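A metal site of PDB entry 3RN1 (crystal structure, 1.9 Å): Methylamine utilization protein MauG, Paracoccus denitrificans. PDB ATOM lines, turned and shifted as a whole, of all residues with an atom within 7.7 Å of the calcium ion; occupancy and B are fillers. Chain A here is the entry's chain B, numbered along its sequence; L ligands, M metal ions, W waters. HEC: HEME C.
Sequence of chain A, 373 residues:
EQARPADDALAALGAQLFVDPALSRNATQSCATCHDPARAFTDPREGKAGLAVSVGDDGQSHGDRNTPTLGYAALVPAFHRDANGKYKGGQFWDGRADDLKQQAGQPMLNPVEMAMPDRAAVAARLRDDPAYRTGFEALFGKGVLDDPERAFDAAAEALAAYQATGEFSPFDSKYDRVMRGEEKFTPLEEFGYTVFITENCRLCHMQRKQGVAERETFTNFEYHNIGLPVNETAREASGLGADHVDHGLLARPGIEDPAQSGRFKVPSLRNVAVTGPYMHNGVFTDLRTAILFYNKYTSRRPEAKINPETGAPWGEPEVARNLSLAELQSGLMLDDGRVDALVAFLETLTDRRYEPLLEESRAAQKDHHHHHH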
ATOM      1  N   ARG A  39     -19.443 -33.286   2.590  1.00  0.00           N
ATOM      2  CA  ARG A  39     -19.657 -32.179   3.510  1.00  0.00           C
ATOM      3  C   ARG A  39     -20.342 -32.672   4.768  1.00  0.00           C
ATOM      4  O   ARG A  39     -21.243 -31.997   5.318  1.00  0.00           O
ATOM      5  CB  ARG A  39     -20.465 -31.041   2.847  1.00  0.00           C
ATOM      6  CG  ARG A  39     -20.362 -29.704   3.573  1.00  0.00           C
ATOM      7  CD  ARG A  39     -21.325 -28.687   2.964  1.00  0.00           C
ATOM      8  NE  ARG A  39     -21.004 -27.296   3.376  1.00  0.00           N
ATOM      9  CZ  ARG A  39     -21.542 -26.655   4.412  1.00  0.00           C
ATOM     10  NH1 ARG A  39     -21.180 -25.414   4.684  1.00  0.00           N
ATOM     11  NH2 ARG A  39     -22.416 -27.258   5.228  1.00  0.00           N
ATOM     12  N   THR A  42     -24.215 -32.844   4.662  1.00  0.00           N
ATOM     13  CA  THR A  42     -25.062 -31.584   4.702  1.00  0.00           C
ATOM     14  C   THR A  42     -25.009 -30.968   3.307  1.00  0.00           C
ATOM     15  O   THR A  42     -24.369 -31.554   2.433  1.00  0.00           O
ATOM     16  CB  THR A  42     -24.573 -30.543   5.751  1.00  0.00           C
ATOM     17  OG1 THR A  42     -23.222 -30.189   5.401  1.00  0.00           O
ATOM     18  CG2 THR A  42     -24.614 -31.202   7.150  1.00  0.00           C
ATOM     19  N   ASP A  43     -25.619 -29.800   3.103  1.00  0.00           N
ATOM     20  CA  ASP A  43     -25.905 -29.286   1.748  1.00  0.00           C
ATOM     21  C   ASP A  43     -24.973 -28.152   1.370  1.00  0.00           C
ATOM     22  O   ASP A  43     -25.086 -27.067   1.956  1.00  0.00           O
ATOM     23  CB  ASP A  43     -27.394 -28.890   1.611  1.00  0.00           C
ATOM     24  CG  ASP A  43     -27.821 -28.634   0.136  1.00  0.00           C
ATOM     25  OD1 ASP A  43     -29.054 -28.385  -0.101  1.00  0.00           O
ATOM     26  OD2 ASP A  43     -26.943 -28.648  -0.798  1.00  0.00           O
ATOM     27  N   LEU A  51     -26.752 -20.908   2.282  1.00  0.00           N
ATOM     28  CA  LEU A  51     -26.788 -22.319   2.676  1.00  0.00           C
ATOM     29  C   LEU A  51     -27.748 -22.655   3.826  1.00  0.00           C
ATOM     30  O   LEU A  51     -27.720 -23.750   4.379  1.00  0.00           O
ATOM     31  CB  LEU A  51     -25.384 -22.786   3.075  1.00  0.00           C
ATOM     32  CG  LEU A  51     -24.443 -23.237   1.924  1.00  0.00           C
ATOM     33  CD1 LEU A  51     -24.068 -22.119   1.053  1.00  0.00           C
ATOM     34  CD2 LEU A  51     -23.186 -23.801   2.505  1.00  0.00           C
ATOM     35  N   ALA A  52     -28.573 -21.700   4.227  1.00  0.00           N
ATOM     36  CA  ALA A  52     -29.432 -21.904   5.408  1.00  0.00           C
ATOM     37  C   ALA A  52     -30.490 -22.972   5.117  1.00  0.00           C
ATOM     38  O   ALA A  52     -30.811 -23.707   6.010  1.00  0.00           O
ATOM     39  CB  ALA A  52     -30.131 -20.599   5.775  1.00  0.00           C
ATOM     40  N   ASN A  66     -32.766 -25.851   8.209  1.00  0.00           N
ATOM     41  CA  ASN A  66     -31.459 -26.199   7.743  1.00  0.00           C
ATOM     42  C   ASN A  66     -31.287 -27.739   7.688  1.00  0.00           C
ATOM     43  O   ASN A  66     -31.784 -28.507   8.541  1.00  0.00           O
ATOM     44  CB  ASN A  66     -30.416 -25.541   8.684  1.00  0.00           C
ATOM     45  CG  ASN A  66     -28.981 -25.832   8.298  1.00  0.00           C
ATOM     46  OD1 ASN A  66     -28.248 -26.540   9.015  1.00  0.00           O
ATOM     47  ND2 ASN A  66     -28.555 -25.273   7.146  1.00  0.00           N
ATOM     48  N   THR A  67     -30.632 -28.189   6.634  1.00  0.00           N
ATOM     49  CA  THR A  67     -30.440 -29.633   6.436  1.00  0.00           C
ATOM     50  C   THR A  67     -29.365 -30.094   7.425  1.00  0.00           C
ATOM     51  O   THR A  67     -28.195 -29.681   7.297  1.00  0.00           O
ATOM     52  CB  THR A  67     -30.052 -29.923   4.988  1.00  0.00           C
ATOM     53  OG1 THR A  67     -31.142 -29.614   4.094  1.00  0.00           O
ATOM     54  CG2 THR A  67     -29.545 -31.323   4.810  1.00  0.00           C
ATOM     55  N   PRO A  68     -29.723 -31.019   8.340  1.00  0.00           N
ATOM     56  CA  PRO A  68     -28.752 -31.467   9.349  1.00  0.00           C
ATOM     57  C   PRO A  68     -27.849 -32.579   8.804  1.00  0.00           C
ATOM     58  O   PRO A  68     -28.225 -33.265   7.822  1.00  0.00           O
ATOM     59  CB  PRO A  68     -29.649 -32.008  10.480  1.00  0.00           C
ATOM     60  CG  PRO A  68     -30.896 -32.626   9.676  1.00  0.00           C
ATOM     61  CD  PRO A  68     -31.097 -31.571   8.565  1.00  0.00           C
ATOM     62  N   THR A  69     -26.730 -32.805   9.469  1.00  0.00           N
ATOM     63  CA  THR A  69     -25.879 -33.940   9.183  1.00  0.00           C
ATOM     64  C   THR A  69     -26.642 -35.220   9.487  1.00  0.00           C
ATOM     65  O   THR A  69     -27.457 -35.284  10.428  1.00  0.00           O
ATOM     66  CB  THR A  69     -24.568 -33.892  10.021  1.00  0.00           C
ATOM     67  OG1 THR A  69     -23.722 -34.971   9.641  1.00  0.00           O
ATOM     68  CG2 THR A  69     -24.853 -34.056  11.575  1.00  0.00           C
ATOM     69  N   TRP A  93     -35.680 -31.954  13.308  1.00  0.00           N
ATOM     70  CA  TRP A  93     -35.375 -30.969  14.332  1.00  0.00           C
ATOM     71  C   TRP A  93     -36.520 -30.964  15.371  1.00  0.00           C
ATOM     72  O   TRP A  93     -36.292 -30.565  16.523  1.00  0.00           O
ATOM     73  CB  TRP A  93     -35.234 -29.562  13.747  1.00  0.00           C
ATOM     74  CG  TRP A  93     -33.877 -29.298  12.957  1.00  0.00           C
ATOM     75  CD1 TRP A  93     -33.669 -29.355  11.620  1.00  0.00           C
ATOM     76  CD2 TRP A  93     -32.639 -28.908  13.537  1.00  0.00           C
ATOM     77  NE1 TRP A  93     -32.357 -29.038  11.315  1.00  0.00           N
ATOM     78  CE2 TRP A  93     -31.706 -28.733  12.462  1.00  0.00           C
ATOM     79  CE3 TRP A  93     -32.244 -28.602  14.855  1.00  0.00           C
ATOM     80  CZ2 TRP A  93     -30.405 -28.302  12.677  1.00  0.00           C
ATOM     81  CZ3 TRP A  93     -30.931 -28.150  15.069  1.00  0.00           C
ATOM     82  CH2 TRP A  93     -30.015 -28.041  13.976  1.00  0.00           C
ATOM     83  N   VAL A 272     -19.555 -30.360  13.919  1.00  0.00           N
ATOM     84  CA  VAL A 272     -20.132 -28.954  13.910  1.00  0.00           C
ATOM     85  C   VAL A 272     -19.250 -27.925  13.205  1.00  0.00           C
ATOM     86  O   VAL A 272     -19.758 -26.983  12.570  1.00  0.00           O
ATOM     87  CB  VAL A 272     -20.482 -28.473  15.299  1.00  0.00           C
ATOM     88  CG1 VAL A 272     -19.214 -28.202  16.182  1.00  0.00           C
ATOM     89  CG2 VAL A 272     -21.406 -27.276  15.220  1.00  0.00           C
ATOM     90  N   VAL A 274     -17.735 -28.169  10.506  1.00  0.00           N
ATOM     91  CA  VAL A 274     -17.795 -28.181   9.050  1.00  0.00           C
ATOM     92  C   VAL A 274     -19.249 -28.179   8.526  1.00  0.00           C
ATOM     93  O   VAL A 274     -19.472 -28.292   7.323  1.00  0.00           O
ATOM     94  CB  VAL A 274     -16.986 -29.336   8.454  1.00  0.00           C
ATOM     95  CG1 VAL A 274     -15.471 -29.286   8.914  1.00  0.00           C
ATOM     96  CG2 VAL A 274     -17.638 -30.630   8.810  1.00  0.00           C
ATOM     97  N   THR A 275     -20.224 -27.971   9.413  1.00  0.00           N
ATOM     98  CA  THR A 275     -21.626 -28.101   8.929  1.00  0.00           C
ATOM     99  C   THR A 275     -22.396 -26.820   9.045  1.00  0.00           C
ATOM    100  O   THR A 275     -23.641 -26.834   9.163  1.00  0.00           O
ATOM    101  CB  THR A 275     -22.380 -29.174   9.648  1.00  0.00           C
ATOM    102  OG1 THR A 275     -22.350 -28.906  11.082  1.00  0.00           O
ATOM    103  CG2 THR A 275     -21.773 -30.534   9.310  1.00  0.00           C
ATOM    104  N   GLY A 276     -21.689 -25.692   8.999  1.00  0.00           N
ATOM    105  CA  GLY A 276     -22.383 -24.370   8.999  1.00  0.00           C
ATOM    106  C   GLY A 276     -23.288 -24.258   7.758  1.00  0.00           C
ATOM    107  O   GLY A 276     -23.098 -25.038   6.795  1.00  0.00           O
ATOM    108  N   PRO A 277     -24.278 -23.321   7.767  1.00  0.00           N
ATOM    109  CA  PRO A 277     -24.558 -22.425   8.886  1.00  0.00           C
ATOM    110  C   PRO A 277     -25.341 -23.189  10.025  1.00  0.00           C
ATOM    111  O   PRO A 277     -25.661 -24.371   9.860  1.00  0.00           O
ATOM    112  CB  PRO A 277     -25.440 -21.328   8.256  1.00  0.00           C
ATOM    113  CG  PRO A 277     -26.239 -22.077   7.189  1.00  0.00           C
ATOM    114  CD  PRO A 277     -25.114 -22.998   6.587  1.00  0.00           C
ATOM    115  N   TYR A 278     -25.647 -22.485  11.110  1.00  0.00           N
ATOM    116  CA  TYR A 278     -25.979 -23.154  12.375  1.00  0.00           C
ATOM    117  C   TYR A 278     -27.403 -22.923  12.823  1.00  0.00           C
ATOM    118  O   TYR A 278     -28.003 -21.958  12.333  1.00  0.00           O
ATOM    119  CB  TYR A 278     -25.006 -22.723  13.455  1.00  0.00           C
ATOM    120  CG  TYR A 278     -23.627 -23.180  13.064  1.00  0.00           C
ATOM    121  CD1 TYR A 278     -22.729 -22.297  12.452  1.00  0.00           C
ATOM    122  CD2 TYR A 278     -23.286 -24.554  13.106  1.00  0.00           C
ATOM    123  CE1 TYR A 278     -21.477 -22.707  12.010  1.00  0.00           C
ATOM    124  CE2 TYR A 278     -21.988 -24.972  12.648  1.00  0.00           C
ATOM    125  CZ  TYR A 278     -21.115 -24.034  12.142  1.00  0.00           C
ATOM    126  OH  TYR A 278     -19.900 -24.423  11.684  1.00  0.00           O
ATOM    127  N   MET A 279     -27.884 -23.773  13.765  1.00  0.00           N
ATOM    128  CA  MET A 279     -29.279 -23.819  14.285  1.00  0.00           C
ATOM    129  C   MET A 279     -30.275 -24.319  13.247  1.00  0.00           C
ATOM    130  O   MET A 279     -29.969 -24.488  12.036  1.00  0.00           O
ATOM    131  CB  MET A 279     -29.717 -22.459  14.802  1.00  0.00           C
ATOM    132  CG  MET A 279     -28.702 -21.803  15.766  1.00  0.00           C
ATOM    133  SD  MET A 279     -28.379 -22.903  17.198  1.00  0.00           S
ATOM    134  CE  MET A 279     -27.055 -21.979  18.052  1.00  0.00           C
ATOM    135  N   HIS A 280     -31.501 -24.519  13.721  1.00  0.00           N
ATOM    136  CA  HIS A 280     -32.520 -25.227  12.968  1.00  0.00           C
ATOM    137  C   HIS A 280     -32.911 -24.472  11.724  1.00  0.00           C
ATOM    138  O   HIS A 280     -33.473 -25.083  10.789  1.00  0.00           O
ATOM    139  CB  HIS A 280     -33.763 -25.497  13.842  1.00  0.00           C
ATOM    140  CG  HIS A 280     -34.523 -24.285  14.191  1.00  0.00           C
ATOM    141  ND1 HIS A 280     -34.387 -23.666  15.411  1.00  0.00           N
ATOM    142  CD2 HIS A 280     -35.398 -23.518  13.475  1.00  0.00           C
ATOM    143  CE1 HIS A 280     -35.116 -22.563  15.429  1.00  0.00           C
ATOM    144  NE2 HIS A 280     -35.767 -22.479  14.283  1.00  0.00           N
ATOM    145  N   ASN A 281     -32.662 -23.149  11.700  1.00  0.00           N
ATOM    146  CA  ASN A 281     -32.946 -22.354  10.510  1.00  0.00           C
ATOM    147  C   ASN A 281     -31.684 -21.787   9.853  1.00  0.00           C
ATOM    148  O   ASN A 281     -31.794 -20.790   9.094  1.00  0.00           O
ATOM    149  CB  ASN A 281     -33.877 -21.183  10.826  1.00  0.00           C
ATOM    150  CG  ASN A 281     -33.377 -20.354  11.998  1.00  0.00           C
ATOM    151  OD1 ASN A 281     -32.204 -20.442  12.366  1.00  0.00           O
ATOM    152  ND2 ASN A 281     -34.260 -19.575  12.602  1.00  0.00           N
ATOM    153  N   GLY A 282     -30.505 -22.345  10.175  1.00  0.00           N
ATOM    154  CA  GLY A 282     -29.261 -21.848   9.490  1.00  0.00           C
ATOM    155  C   GLY A 282     -29.004 -20.353   9.711  1.00  0.00           C
ATOM    156  O   GLY A 282     -28.374 -19.706   8.873  1.00  0.00           O
ATOM    157  N   PHE A 284     -27.099 -18.496  11.771  1.00  0.00           N
ATOM    158  CA  PHE A 284     -25.722 -17.999  12.009  1.00  0.00           C
ATOM    159  C   PHE A 284     -24.779 -18.656  11.060  1.00  0.00           C
ATOM    160  O   PHE A 284     -24.735 -19.902  11.034  1.00  0.00           O
ATOM    161  CB  PHE A 284     -25.302 -18.332  13.438  1.00  0.00           C
ATOM    162  CG  PHE A 284     -26.218 -17.787  14.460  1.00  0.00           C
ATOM    163  CD1 PHE A 284     -26.757 -16.496  14.326  1.00  0.00           C
ATOM    164  CD2 PHE A 284     -26.519 -18.534  15.599  1.00  0.00           C
ATOM    165  CE1 PHE A 284     -27.639 -15.972  15.304  1.00  0.00           C
ATOM    166  CE2 PHE A 284     -27.365 -18.017  16.573  1.00  0.00           C
ATOM    167  CZ  PHE A 284     -27.939 -16.730  16.426  1.00  0.00           C
HETATM  168 FE   HEC L   1     -26.133 -25.513  22.234  1.00  0.00          FE
HETATM  169  CHA HEC L   1     -27.291 -25.690  18.975  1.00  0.00           C
HETATM  170  CHB HEC L   1     -22.976 -25.022  21.077  1.00  0.00           C
HETATM  171  CHC HEC L   1     -25.145 -24.628  25.400  1.00  0.00           C
HETATM  172  CHD HEC L   1     -29.081 -26.603  23.442  1.00  0.00           C
HETATM  173  NA  HEC L   1     -25.280 -25.363  20.351  1.00  0.00           N
HETATM  174  C1A HEC L   1     -25.847 -25.510  19.169  1.00  0.00           C
HETATM  175  C2A HEC L   1     -24.921 -25.276  18.046  1.00  0.00           C
HETATM  176  C3A HEC L   1     -23.690 -25.108  18.612  1.00  0.00           C
HETATM  177  C4A HEC L   1     -24.001 -25.177  20.067  1.00  0.00           C
HETATM  178  CMA HEC L   1     -22.319 -24.860  17.986  1.00  0.00           C
HETATM  179  CAA HEC L   1     -25.327 -25.346  16.600  1.00  0.00           C
HETATM  180  CBA HEC L   1     -25.216 -26.849  16.233  1.00  0.00           C
HETATM  181  CGA HEC L   1     -25.809 -27.032  14.822  1.00  0.00           C
HETATM  182  O1A HEC L   1     -26.510 -26.137  14.286  1.00  0.00           O
HETATM  183  O2A HEC L   1     -25.650 -28.137  14.241  1.00  0.00           O
HETATM  184  NB  HEC L   1     -24.389 -24.959  23.068  1.00  0.00           N
HETATM  185  C1B HEC L   1     -23.201 -24.808  22.479  1.00  0.00           C
HETATM  186  C2B HEC L   1     -22.107 -24.415  23.366  1.00  0.00           C
HETATM  187  C3B HEC L   1     -22.769 -24.289  24.578  1.00  0.00           C
HETATM  188  C4B HEC L   1     -24.152 -24.618  24.328  1.00  0.00           C
HETATM  189  CMB HEC L   1     -20.635 -24.239  22.961  1.00  0.00           C
HETATM  190  CAB HEC L   1     -22.261 -23.814  25.952  1.00  0.00           C
HETATM  191  CBB HEC L   1     -21.904 -22.331  25.714  1.00  0.00           C
HETATM  192  NC  HEC L   1     -26.962 -25.659  24.080  1.00  0.00           N
HETATM  193  C1C HEC L   1     -26.485 -25.166  25.227  1.00  0.00           C
HETATM  194  C2C HEC L   1     -27.409 -25.359  26.348  1.00  0.00           C
HETATM  195  C3C HEC L   1     -28.536 -25.943  25.781  1.00  0.00           C
HETATM  196  C4C HEC L   1     -28.182 -26.070  24.381  1.00  0.00           C
HETATM  197  CMC HEC L   1     -27.152 -25.002  27.814  1.00  0.00           C
HETATM  198  CAC HEC L   1     -29.817 -26.405  26.430  1.00  0.00           C
HETATM  199  CBC HEC L   1     -30.460 -25.409  27.340  1.00  0.00           C
HETATM  200  ND  HEC L   1     -27.858 -26.055  21.358  1.00  0.00           N
HETATM  201  C1D HEC L   1     -28.986 -26.399  21.991  1.00  0.00           C
HETATM  202  C2D HEC L   1     -30.130 -26.570  21.114  1.00  0.00           C
HETATM  203  C3D HEC L   1     -29.607 -26.282  19.854  1.00  0.00           C
HETATM  204  C4D HEC L   1     -28.208 -25.964  20.053  1.00  0.00           C
HETATM  205  CMD HEC L   1     -31.557 -26.941  21.492  1.00  0.00           C
HETATM  206  CAD HEC L   1     -30.397 -26.273  18.592  1.00  0.00           C
HETATM  207  CBD HEC L   1     -31.202 -24.961  18.769  1.00  0.00           C
HETATM  208  CGD HEC L   1     -32.088 -24.742  17.544  1.00  0.00           C
HETATM  209  O1D HEC L   1     -31.600 -24.773  16.378  1.00  0.00           O
HETATM  210  O2D HEC L   1     -33.318 -24.541  17.741  1.00  0.00           O
HETATM  211 CA    CA M   1     -25.918 -26.717   9.727  1.00  0.00          CA
HETATM  212  O   HOH W   1     -25.743 -26.446   7.326  1.00  0.00           O
HETATM  213  O   HOH W   2     -27.384 -26.483  11.617  1.00  0.00           O
HETATM  214  O   HOH W   3     -24.857 -27.590  11.604  1.00  0.00           O
HETATM  215  O   HOH W   4     -26.193 -28.889   9.221  1.00  0.00           O
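The backbone carbonyl oxygen (O) of Asn 66 lies within hydrogen-bond range of the indole nitrogen (NE1) of Trp 93, at 2.9 Å.
The side-chain amide nitrogen (ND2) of Asn 66 is in hydrogen-bond range of the backbone carbonyl oxygen (O) of Leu 51.
O of Ala 52 lies within hydrogen-bond range of ND2 of Asn 66 (3.0 Å).
The backbone carbonyl oxygen (O) of His 280 lies within hydrogen-bond range of the backbone NH (N) of Asn 66.
Three residues have an atom within 4 Å of the calcium ion: Asn 66, Thr 275 and Pro 277.
The nearest printed residue that does not touch the calcium ion is Gly 276 (4.1 Å).
Water W2 bridges an oxygen (O1A) of the ligand (2.8 Å) and the backbone carbonyl oxygen of Met 279 (3.3 Å).
Water W3 lies within hydrogen-bond range of an oxygen (O2A) of the ligand (2.8 Å) and the side-chain hydroxyl (OG1) of Thr 275 (2.9 Å).
Water W1 lies within hydrogen-bond range of the backbone carbonyl oxygen of Gly 276 (3.0 Å) and the side-chain amide nitrogen of Asn 66 (3.1 Å).
The calcium ion is bound by water W4, water W3, the backbone carbonyl oxygen (O) of Thr 275, the backbone carbonyl oxygen (O) of Pro 277, water W2, water W1 and the side-chain amide oxygen (OD1) of Asn 66.
The calcium ion has seven donor atoms within binding distance.
The backbone NH (N) of Met 279 sits at hydrogen-bond distance from an oxygen (O1A) of the ligand (2.8 Å).
The backbone NH of His 280 sits at hydrogen-bond distance from an oxygen (O1D) of the ligand.
A ring nitrogen (ND1) of His 280 sits at hydrogen-bond distance from an oxygen (O2D) of the ligand, at 2.7 Å.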
